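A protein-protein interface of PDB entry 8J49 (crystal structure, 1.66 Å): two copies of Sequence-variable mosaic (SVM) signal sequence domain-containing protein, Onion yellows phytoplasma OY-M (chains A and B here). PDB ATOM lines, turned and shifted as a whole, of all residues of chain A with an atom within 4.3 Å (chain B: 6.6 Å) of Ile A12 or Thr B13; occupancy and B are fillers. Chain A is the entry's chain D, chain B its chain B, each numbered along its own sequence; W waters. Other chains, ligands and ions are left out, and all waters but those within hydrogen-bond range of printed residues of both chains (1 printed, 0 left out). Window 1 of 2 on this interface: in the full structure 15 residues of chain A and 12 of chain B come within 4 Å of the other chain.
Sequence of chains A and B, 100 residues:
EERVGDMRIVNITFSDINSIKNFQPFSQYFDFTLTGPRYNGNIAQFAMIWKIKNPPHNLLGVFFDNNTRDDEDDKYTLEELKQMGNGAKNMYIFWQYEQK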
ATOM      1  N   VAL A  10      21.972 -12.361 -19.963  1.00  0.00           N
ATOM      2  CA  VAL A  10      22.939 -11.574 -19.197  1.00  0.00           C
ATOM      3  C   VAL A  10      22.922 -10.167 -19.759  1.00  0.00           C
ATOM      4  O   VAL A  10      23.447  -9.936 -20.855  1.00  0.00           O
ATOM      5  CB  VAL A  10      24.353 -12.160 -19.308  1.00  0.00           C
ATOM      6  CG1 VAL A  10      25.321 -11.393 -18.420  1.00  0.00           C
ATOM      7  CG2 VAL A  10      24.355 -13.634 -18.982  1.00  0.00           C
ATOM      8  N   ASN A  11      22.359  -9.221 -19.007  1.00  0.00           N
ATOM      9  CA  ASN A  11      22.373  -7.811 -19.383  1.00  0.00           C
ATOM     10  C   ASN A  11      23.634  -7.154 -18.835  1.00  0.00           C
ATOM     11  O   ASN A  11      23.846  -7.141 -17.619  1.00  0.00           O
ATOM     12  CB  ASN A  11      21.141  -7.097 -18.827  1.00  0.00           C
ATOM     13  CG  ASN A  11      19.861  -7.605 -19.426  1.00  0.00           C
ATOM     14  OD1 ASN A  11      19.487  -7.209 -20.527  1.00  0.00           O
ATOM     15  ND2 ASN A  11      19.164  -8.478 -18.696  1.00  0.00           N
ATOM     16  N   ILE A  12      24.451  -6.581 -19.718  1.00  0.00           N
ATOM     17  CA  ILE A  12      25.659  -5.863 -19.315  1.00  0.00           C
ATOM     18  C   ILE A  12      25.545  -4.422 -19.791  1.00  0.00           C
ATOM     19  O   ILE A  12      25.192  -4.174 -20.950  1.00  0.00           O
ATOM     20  CB  ILE A  12      26.922  -6.547 -19.872  1.00  0.00           C
ATOM     21  CG1 ILE A  12      26.871  -8.045 -19.579  1.00  0.00           C
ATOM     22  CG2 ILE A  12      28.186  -5.923 -19.274  1.00  0.00           C
ATOM     23  CD1 ILE A  12      28.025  -8.842 -20.174  1.00  0.00           C
ATOM     24  N   THR A  13      25.826  -3.472 -18.897  1.00  0.00           N
ATOM     25  CA  THR A  13      25.739  -2.055 -19.211  1.00  0.00           C
ATOM     26  C   THR A  13      27.139  -1.466 -19.202  1.00  0.00           C
ATOM     27  O   THR A  13      27.905  -1.684 -18.253  1.00  0.00           O
ATOM     28  CB  THR A  13      24.839  -1.325 -18.214  1.00  0.00           C
ATOM     29  OG1 THR A  13      23.501  -1.824 -18.341  1.00  0.00           O
ATOM     30  CG2 THR A  13      24.843   0.174 -18.479  1.00  0.00           C
ATOM     31  N   PHE A  14      27.471  -0.733 -20.259  1.00  0.00           N
ATOM     32  CA  PHE A  14      28.811  -0.218 -20.477  1.00  0.00           C
ATOM     33  C   PHE A  14      28.814   1.300 -20.466  1.00  0.00           C
ATOM     34  O   PHE A  14      27.778   1.947 -20.638  1.00  0.00           O
ATOM     35  CB  PHE A  14      29.394  -0.684 -21.817  1.00  0.00           C
ATOM     36  CG  PHE A  14      29.497  -2.167 -21.951  1.00  0.00           C
ATOM     37  CD1 PHE A  14      28.401  -2.912 -22.367  1.00  0.00           C
ATOM     38  CD2 PHE A  14      30.681  -2.819 -21.666  1.00  0.00           C
ATOM     39  CE1 PHE A  14      28.486  -4.293 -22.503  1.00  0.00           C
ATOM     40  CE2 PHE A  14      30.775  -4.200 -21.805  1.00  0.00           C
ATOM     41  CZ  PHE A  14      29.678  -4.937 -22.231  1.00  0.00           C
ATOM     42  N   PHE A  23      37.128  -5.740 -24.228  1.00  0.00           N
ATOM     43  CA  PHE A  23      36.418  -6.856 -23.608  1.00  0.00           C
ATOM     44  C   PHE A  23      36.706  -8.127 -24.390  1.00  0.00           C
ATOM     45  O   PHE A  23      36.130  -8.356 -25.459  1.00  0.00           O
ATOM     46  CB  PHE A  23      34.918  -6.582 -23.582  1.00  0.00           C
ATOM     47  CG  PHE A  23      34.390  -6.190 -22.238  1.00  0.00           C
ATOM     48  CD1 PHE A  23      34.365  -4.859 -21.867  1.00  0.00           C
ATOM     49  CD2 PHE A  23      33.837  -7.134 -21.390  1.00  0.00           C
ATOM     50  CE1 PHE A  23      33.882  -4.470 -20.635  1.00  0.00           C
ATOM     51  CE2 PHE A  23      33.326  -6.758 -20.162  1.00  0.00           C
ATOM     52  CZ  PHE A  23      33.349  -5.416 -19.783  1.00  0.00           C
ATOM     53  N   PHE A  26      33.879 -10.594 -26.105  1.00  0.00           N
ATOM     54  CA  PHE A  26      32.836  -9.915 -26.919  1.00  0.00           C
ATOM     55  C   PHE A  26      33.376  -8.987 -28.007  1.00  0.00           C
ATOM     56  O   PHE A  26      32.618  -8.763 -28.969  1.00  0.00           O
ATOM     57  CB  PHE A  26      31.891  -9.128 -26.008  1.00  0.00           C
ATOM     58  CG  PHE A  26      31.456  -9.877 -24.775  1.00  0.00           C
ATOM     59  CD1 PHE A  26      30.839 -11.112 -24.877  1.00  0.00           C
ATOM     60  CD2 PHE A  26      31.665  -9.343 -23.514  1.00  0.00           C
ATOM     61  CE1 PHE A  26      30.443 -11.800 -23.742  1.00  0.00           C
ATOM     62  CE2 PHE A  26      31.264 -10.030 -22.381  1.00  0.00           C
ATOM     63  CZ  PHE A  26      30.654 -11.257 -22.498  1.00  0.00           C
ATOM     64  N   TYR A  92      23.961 -12.627 -24.336  1.00  0.00           N
ATOM     65  CA  TYR A  92      24.465 -11.383 -23.760  1.00  0.00           C
ATOM     66  C   TYR A  92      23.794 -10.208 -24.453  1.00  0.00           C
ATOM     67  O   TYR A  92      23.769 -10.140 -25.688  1.00  0.00           O
ATOM     68  CB  TYR A  92      25.987 -11.285 -23.898  1.00  0.00           C
ATOM     69  CG  TYR A  92      26.710 -12.428 -23.234  1.00  0.00           C
ATOM     70  CD1 TYR A  92      27.034 -12.367 -21.877  1.00  0.00           C
ATOM     71  CD2 TYR A  92      27.066 -13.572 -23.953  1.00  0.00           C
ATOM     72  CE1 TYR A  92      27.679 -13.416 -21.254  1.00  0.00           C
ATOM     73  CE2 TYR A  92      27.717 -14.632 -23.334  1.00  0.00           C
ATOM     74  CZ  TYR A  92      28.030 -14.534 -21.979  1.00  0.00           C
ATOM     75  OH  TYR A  92      28.673 -15.565 -21.337  1.00  0.00           O
ATOM     76  N   ILE A  93      23.215  -9.317 -23.661  1.00  0.00           N
ATOM     77  CA  ILE A  93      22.541  -8.120 -24.151  1.00  0.00           C
ATOM     78  C   ILE A  93      23.335  -6.908 -23.666  1.00  0.00           C
ATOM     79  O   ILE A  93      23.431  -6.659 -22.455  1.00  0.00           O
ATOM     80  CB  ILE A  93      21.078  -8.056 -23.676  1.00  0.00           C
ATOM     81  CG1 ILE A  93      20.305  -9.296 -24.133  1.00  0.00           C
ATOM     82  CG2 ILE A  93      20.410  -6.805 -24.245  1.00  0.00           C
ATOM     83  CD1 ILE A  93      18.833  -9.309 -23.653  1.00  0.00           C
ATOM     84  N   PHE A  94      23.890  -6.151 -24.610  1.00  0.00           N
ATOM     85  CA  PHE A  94      24.825  -5.068 -24.303  1.00  0.00           C
ATOM     86  C   PHE A  94      24.101  -3.729 -24.363  1.00  0.00           C
ATOM     87  O   PHE A  94      23.453  -3.413 -25.367  1.00  0.00           O
ATOM     88  CB  PHE A  94      25.995  -5.060 -25.289  1.00  0.00           C
ATOM     89  CG  PHE A  94      26.708  -6.380 -25.408  1.00  0.00           C
ATOM     90  CD1 PHE A  94      27.415  -6.911 -24.345  1.00  0.00           C
ATOM     91  CD2 PHE A  94      26.679  -7.084 -26.599  1.00  0.00           C
ATOM     92  CE1 PHE A  94      28.071  -8.123 -24.463  1.00  0.00           C
ATOM     93  CE2 PHE A  94      27.335  -8.290 -26.716  1.00  0.00           C
ATOM     94  CZ  PHE A  94      28.036  -8.807 -25.656  1.00  0.00           C
ATOM     95  N   TRP A  95      24.242  -2.935 -23.302  1.00  0.00           N
ATOM     96  CA  TRP A  95      23.534  -1.676 -23.149  1.00  0.00           C
ATOM     97  C   TRP A  95      24.508  -0.525 -22.941  1.00  0.00           C
ATOM     98  O   TRP A  95      25.586  -0.700 -22.370  1.00  0.00           O
ATOM     99  CB  TRP A  95      22.602  -1.721 -21.941  1.00  0.00           C
ATOM    100  CG  TRP A  95      21.565  -2.787 -22.004  1.00  0.00           C
ATOM    101  CD1 TRP A  95      21.641  -4.034 -21.463  1.00  0.00           C
ATOM    102  CD2 TRP A  95      20.278  -2.694 -22.618  1.00  0.00           C
ATOM    103  NE1 TRP A  95      20.488  -4.726 -21.709  1.00  0.00           N
ATOM    104  CE2 TRP A  95      19.635  -3.925 -22.421  1.00  0.00           C
ATOM    105  CE3 TRP A  95      19.615  -1.692 -23.337  1.00  0.00           C
ATOM    106  CZ2 TRP A  95      18.348  -4.186 -22.895  1.00  0.00           C
ATOM    107  CZ3 TRP A  95      18.335  -1.955 -23.808  1.00  0.00           C
ATOM    108  CH2 TRP A  95      17.719  -3.188 -23.584  1.00  0.00           C
ATOM    109  N   ASN B  11      24.491   0.097 -12.560  1.00  0.00           N
ATOM    110  CA  ASN B  11      25.608  -0.842 -12.547  1.00  0.00           C
ATOM    111  C   ASN B  11      26.309  -0.784 -13.899  1.00  0.00           C
ATOM    112  O   ASN B  11      25.717  -1.150 -14.916  1.00  0.00           O
ATOM    113  CB  ASN B  11      25.105  -2.255 -12.273  1.00  0.00           C
ATOM    114  CG  ASN B  11      24.507  -2.390 -10.896  1.00  0.00           C
ATOM    115  OD1 ASN B  11      25.217  -2.302  -9.897  1.00  0.00           O
ATOM    116  ND2 ASN B  11      23.192  -2.591 -10.833  1.00  0.00           N
ATOM    117  N   ILE B  12      27.563  -0.343 -13.911  1.00  0.00           N
ATOM    118  CA  ILE B  12      28.354  -0.229 -15.127  1.00  0.00           C
ATOM    119  C   ILE B  12      29.520  -1.197 -15.022  1.00  0.00           C
ATOM    120  O   ILE B  12      30.213  -1.234 -13.998  1.00  0.00           O
ATOM    121  CB  ILE B  12      28.859   1.210 -15.350  1.00  0.00           C
ATOM    122  CG1 ILE B  12      27.712   2.209 -15.194  1.00  0.00           C
ATOM    123  CG2 ILE B  12      29.480   1.346 -16.728  1.00  0.00           C
ATOM    124  CD1 ILE B  12      28.121   3.641 -15.523  1.00  0.00           C
ATOM    125  N   THR B  13      29.759  -1.956 -16.096  1.00  0.00           N
ATOM    126  CA  THR B  13      30.737  -3.031 -16.096  1.00  0.00           C
ATOM    127  C   THR B  13      31.911  -2.669 -16.993  1.00  0.00           C
ATOM    128  O   THR B  13      31.727  -2.113 -18.079  1.00  0.00           O
ATOM    129  CB  THR B  13      30.085  -4.352 -16.551  1.00  0.00           C
ATOM    130  OG1 THR B  13      29.011  -4.681 -15.661  1.00  0.00           O
ATOM    131  CG2 THR B  13      31.080  -5.490 -16.531  1.00  0.00           C
ATOM    132  N   PHE B  14      33.111  -2.981 -16.516  1.00  0.00           N
ATOM    133  CA  PHE B  14      34.365  -2.646 -17.165  1.00  0.00           C
ATOM    134  C   PHE B  14      35.230  -3.889 -17.221  1.00  0.00           C
ATOM    135  O   PHE B  14      35.081  -4.809 -16.419  1.00  0.00           O
ATOM    136  CB  PHE B  14      35.125  -1.534 -16.404  1.00  0.00           C
ATOM    137  CG  PHE B  14      34.442  -0.204 -16.449  1.00  0.00           C
ATOM    138  CD1 PHE B  14      33.422   0.085 -15.565  1.00  0.00           C
ATOM    139  CD2 PHE B  14      34.813   0.753 -17.381  1.00  0.00           C
ATOM    140  CE1 PHE B  14      32.776   1.298 -15.611  1.00  0.00           C
ATOM    141  CE2 PHE B  14      34.172   1.973 -17.427  1.00  0.00           C
ATOM    142  CZ  PHE B  14      33.151   2.243 -16.535  1.00  0.00           C
ATOM    143  N   SER B  15      36.168  -3.887 -18.162  1.00  0.00           N
ATOM    144  CA  SER B  15      37.135  -4.977 -18.241  1.00  0.00           C
ATOM    145  C   SER B  15      38.000  -5.043 -16.990  1.00  0.00           C
ATOM    146  O   SER B  15      38.251  -6.127 -16.451  1.00  0.00           O
ATOM    147  CB  SER B  15      38.007  -4.793 -19.479  1.00  0.00           C
ATOM    148  OG  SER B  15      38.712  -5.982 -19.773  1.00  0.00           O
ATOM    149  N   SER B  19      40.412   0.526 -17.337  1.00  0.00           N
ATOM    150  CA  SER B  19      39.472   1.009 -18.340  1.00  0.00           C
ATOM    151  C   SER B  19      38.611   2.144 -17.806  1.00  0.00           C
ATOM    152  O   SER B  19      38.117   2.962 -18.591  1.00  0.00           O
ATOM    153  CB  SER B  19      38.600  -0.146 -18.845  1.00  0.00           C
ATOM    154  OG  SER B  19      37.358   0.334 -19.321  1.00  0.00           O
ATOM    155  N   ILE B  93      27.639   2.304  -9.730  1.00  0.00           N
ATOM    156  CA  ILE B  93      28.351   1.183  -9.141  1.00  0.00           C
ATOM    157  C   ILE B  93      29.198   0.522 -10.217  1.00  0.00           C
ATOM    158  O   ILE B  93      28.669   0.045 -11.227  1.00  0.00           O
ATOM    159  CB  ILE B  93      27.386   0.201  -8.468  1.00  0.00           C
ATOM    160  CG1 ILE B  93      26.397   0.972  -7.557  1.00  0.00           C
ATOM    161  CG2 ILE B  93      28.127  -0.935  -7.773  1.00  0.00           C
ATOM    162  CD1 ILE B  93      25.387   0.067  -6.857  1.00  0.00           C
ATOM    163  N   PHE B  94      30.513   0.498  -9.998  1.00  0.00           N
ATOM    164  CA  PHE B  94      31.463   0.074 -11.023  1.00  0.00           C
ATOM    165  C   PHE B  94      31.911  -1.354 -10.744  1.00  0.00           C
ATOM    166  O   PHE B  94      32.367  -1.663  -9.637  1.00  0.00           O
ATOM    167  CB  PHE B  94      32.670   1.011 -11.062  1.00  0.00           C
ATOM    168  CG  PHE B  94      32.309   2.444 -11.314  1.00  0.00           C
ATOM    169  CD1 PHE B  94      31.848   3.251 -10.274  1.00  0.00           C
ATOM    170  CD2 PHE B  94      32.413   2.991 -12.575  1.00  0.00           C
ATOM    171  CE1 PHE B  94      31.515   4.576 -10.502  1.00  0.00           C
ATOM    172  CE2 PHE B  94      32.079   4.317 -12.805  1.00  0.00           C
ATOM    173  CZ  PHE B  94      31.636   5.114 -11.748  1.00  0.00           C
ATOM    174  N   TRP B  95      31.789  -2.218 -11.755  1.00  0.00           N
ATOM    175  CA  TRP B  95      32.028  -3.645 -11.613  1.00  0.00           C
ATOM    176  C   TRP B  95      33.068  -4.106 -12.615  1.00  0.00           C
ATOM    177  O   TRP B  95      33.123  -3.601 -13.737  1.00  0.00           O
ATOM    178  CB  TRP B  95      30.756  -4.450 -11.857  1.00  0.00           C
ATOM    179  CG  TRP B  95      29.680  -4.180 -10.893  1.00  0.00           C
ATOM    180  CD1 TRP B  95      28.659  -3.289 -11.032  1.00  0.00           C
ATOM    181  CD2 TRP B  95      29.496  -4.820  -9.633  1.00  0.00           C
ATOM    182  NE1 TRP B  95      27.843  -3.337  -9.929  1.00  0.00           N
ATOM    183  CE2 TRP B  95      28.336  -4.272  -9.055  1.00  0.00           C
ATOM    184  CE3 TRP B  95      30.192  -5.820  -8.943  1.00  0.00           C
ATOM    185  CZ2 TRP B  95      27.865  -4.679  -7.819  1.00  0.00           C
ATOM    186  CZ3 TRP B  95      29.728  -6.221  -7.720  1.00  0.00           C
ATOM    187  CH2 TRP B  95      28.568  -5.660  -7.167  1.00  0.00           C
ATOM    188  N   GLN B  96      33.887  -5.064 -12.208  1.00  0.00           N
ATOM    189  CA  GLN B  96      34.781  -5.733 -13.138  1.00  0.00           C
ATOM    190  C   GLN B  96      34.092  -6.985 -13.677  1.00  0.00           C
ATOM    191  O   GLN B  96      33.549  -7.788 -12.908  1.00  0.00           O
ATOM    192  CB  GLN B  96      36.103  -6.080 -12.456  1.00  0.00           C
ATOM    193  CG  GLN B  96      36.979  -7.001 -13.284  1.00  0.00           C
ATOM    194  CD  GLN B  96      38.443  -6.879 -12.964  1.00  0.00           C
ATOM    195  OE1 GLN B  96      38.873  -5.953 -12.268  1.00  0.00           O
ATOM    196  NE2 GLN B  96      39.225  -7.834 -13.441  1.00  0.00           N
ATOM    197  N   TYR B  97      34.089  -7.134 -15.000  1.00  0.00           N
ATOM    198  CA  TYR B  97      33.422  -8.286 -15.593  1.00  0.00           C
ATOM    199  C   TYR B  97      34.145  -9.568 -15.209  1.00  0.00           C
ATOM    200  O   TYR B  97      35.377  -9.628 -15.212  1.00  0.00           O
ATOM    201  CB  TYR B  97      33.369  -8.166 -17.117  1.00  0.00           C
ATOM    202  CG  TYR B  97      32.653  -9.336 -17.769  1.00  0.00           C
ATOM    203  CD1 TYR B  97      31.277  -9.487 -17.644  1.00  0.00           C
ATOM    204  CD2 TYR B  97      33.357 -10.304 -18.467  1.00  0.00           C
ATOM    205  CE1 TYR B  97      30.612 -10.575 -18.227  1.00  0.00           C
ATOM    206  CE2 TYR B  97      32.702 -11.392 -19.046  1.00  0.00           C
ATOM    207  CZ  TYR B  97      31.336 -11.517 -18.921  1.00  0.00           C
ATOM    208  OH  TYR B  97      30.683 -12.592 -19.494  1.00  0.00           O
ATOM    209  N   GLU B  98      33.374 -10.601 -14.874  1.00  0.00           N
ATOM    210  CA  GLU B  98      33.911 -11.952 -14.784  1.00  0.00           C
ATOM    211  C   GLU B  98      33.038 -12.889 -15.612  1.00  0.00           C
ATOM    212  O   GLU B  98      31.815 -12.728 -15.667  1.00  0.00           O
ATOM    213  CB  GLU B  98      33.987 -12.462 -13.337  1.00  0.00           C
ATOM    214  CG  GLU B  98      32.844 -12.065 -12.418  1.00  0.00           C
ATOM    215  CD  GLU B  98      33.074 -12.595 -11.005  1.00  0.00           C
ATOM    216  OE1 GLU B  98      34.141 -13.216 -10.804  1.00  0.00           O
ATOM    217  OE2 GLU B  98      32.196 -12.453 -10.121  1.00  0.00           O
HETATM  218  O   HOH W   1      26.432  -3.867 -16.012  1.00  0.00           O
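The backbone NH of Thr B13 lies within hydrogen-bond range of the backbone carbonyl oxygen of Thr A13 (2.9 Å).
The side-chain amide oxygen (OD1) of Asn B11 is in hydrogen-bond range of the indole nitrogen (NE1) of Trp B95 (2.8 Å). The backbone carbonyl oxygen of Ile B93 lies within hydrogen-bond range of the backbone NH of Ile B12. N of Phe B14 sits at hydrogen-bond distance from O of Trp B95 (2.8 Å). The backbone NH (N) of Tyr B97 sits at hydrogen-bond distance from the backbone carbonyl oxygen (O) of Phe B14 (2.9 Å). The backbone carbonyl oxygen (O) of Ile A12 sits at hydrogen-bond distance from the backbone NH (N) of Trp A95 (2.8 Å). The backbone carbonyl oxygen (O) of Trp A95 is in hydrogen-bond range of the backbone NH (N) of Phe A14, at 2.8 Å.
Among the printed residues, pairs that only touch across the chains: Ile A12 with Thr B13, Ile A12 with Tyr B97, Thr A13 with Asn B11, Thr A13 with Ile B12, Phe A14 with Ile B12, Phe A14 with Thr B13, Phe A23 with Thr B13, Phe A23 with Phe B14, Phe A23 with Ser B15, Phe A23 with Tyr B97, Phe A26 with Tyr B97 and Tyr A92 with Tyr B97.
Of the printed residues of chain B, Ile A12 touches Thr B13 and Tyr B97. Of chain A, only Ile A12, Thr A13, Phe A14 and Phe A23 come within 4 Å of Thr B13. Of the printed residues of chain A, Tyr B97 touches Ile A12, Phe A23, Phe A26 and Tyr A92. Printed residues of chain B within 4 Å of Phe A23: Thr B13 (3.97 Å), Phe B14 (3.5 Å), Ser B15 (3.4 Å) and Tyr B97 (3.4 Å). Trp A95 touches none of the printed residues of chain B. Trp B95 touches none of the printed residues of chain A. The nearest printed residue of chain A that does not touch Thr B13 is Asn A11 (6.0 Å). The nearest printed residue of chain A that does not touch Asn B11 is Phe A14 (5.6 Å).
Hydrophobic or aromatic side chains of chain B within 4 Å of the printed part of chain A: Ile B12 and Tyr B97. Along chain B the printed residues that touch a printed residue of chain A span positions 11 to 97. Printed residues of chain A that touch a printed residue of chain B: Ile A12, Thr A13, Phe A14, Phe A23, Phe A26 and Tyr A92. Hydrophobic or aromatic side chains of chain A within 4 Å of the printed part of chain B: Ile A12, Phe A14, Phe A23, Phe A26 and Tyr A92. Among the printed residues, 13 pairs touch across the chains.
Ile A12 touches Thr B13, and with the chains exchanged Thr A13 touches Ile B12. Thr A13 touches Asn B11, but with the chains exchanged Asn A11 does not touch Thr B13 (6.0 Å). Thr B13 touches its own counterpart, Thr A13. Phe A14 touches Thr B13, but with the chains exchanged Thr A13 does not touch Phe B14 (5.6 Å). 7 positions are printed for both chains.
Water W1 lies within hydrogen-bond range of OG1 of Thr B13 (2.7 Å), N of Thr A13 (3.0 Å) and O of Asn B11 (3.0 Å).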
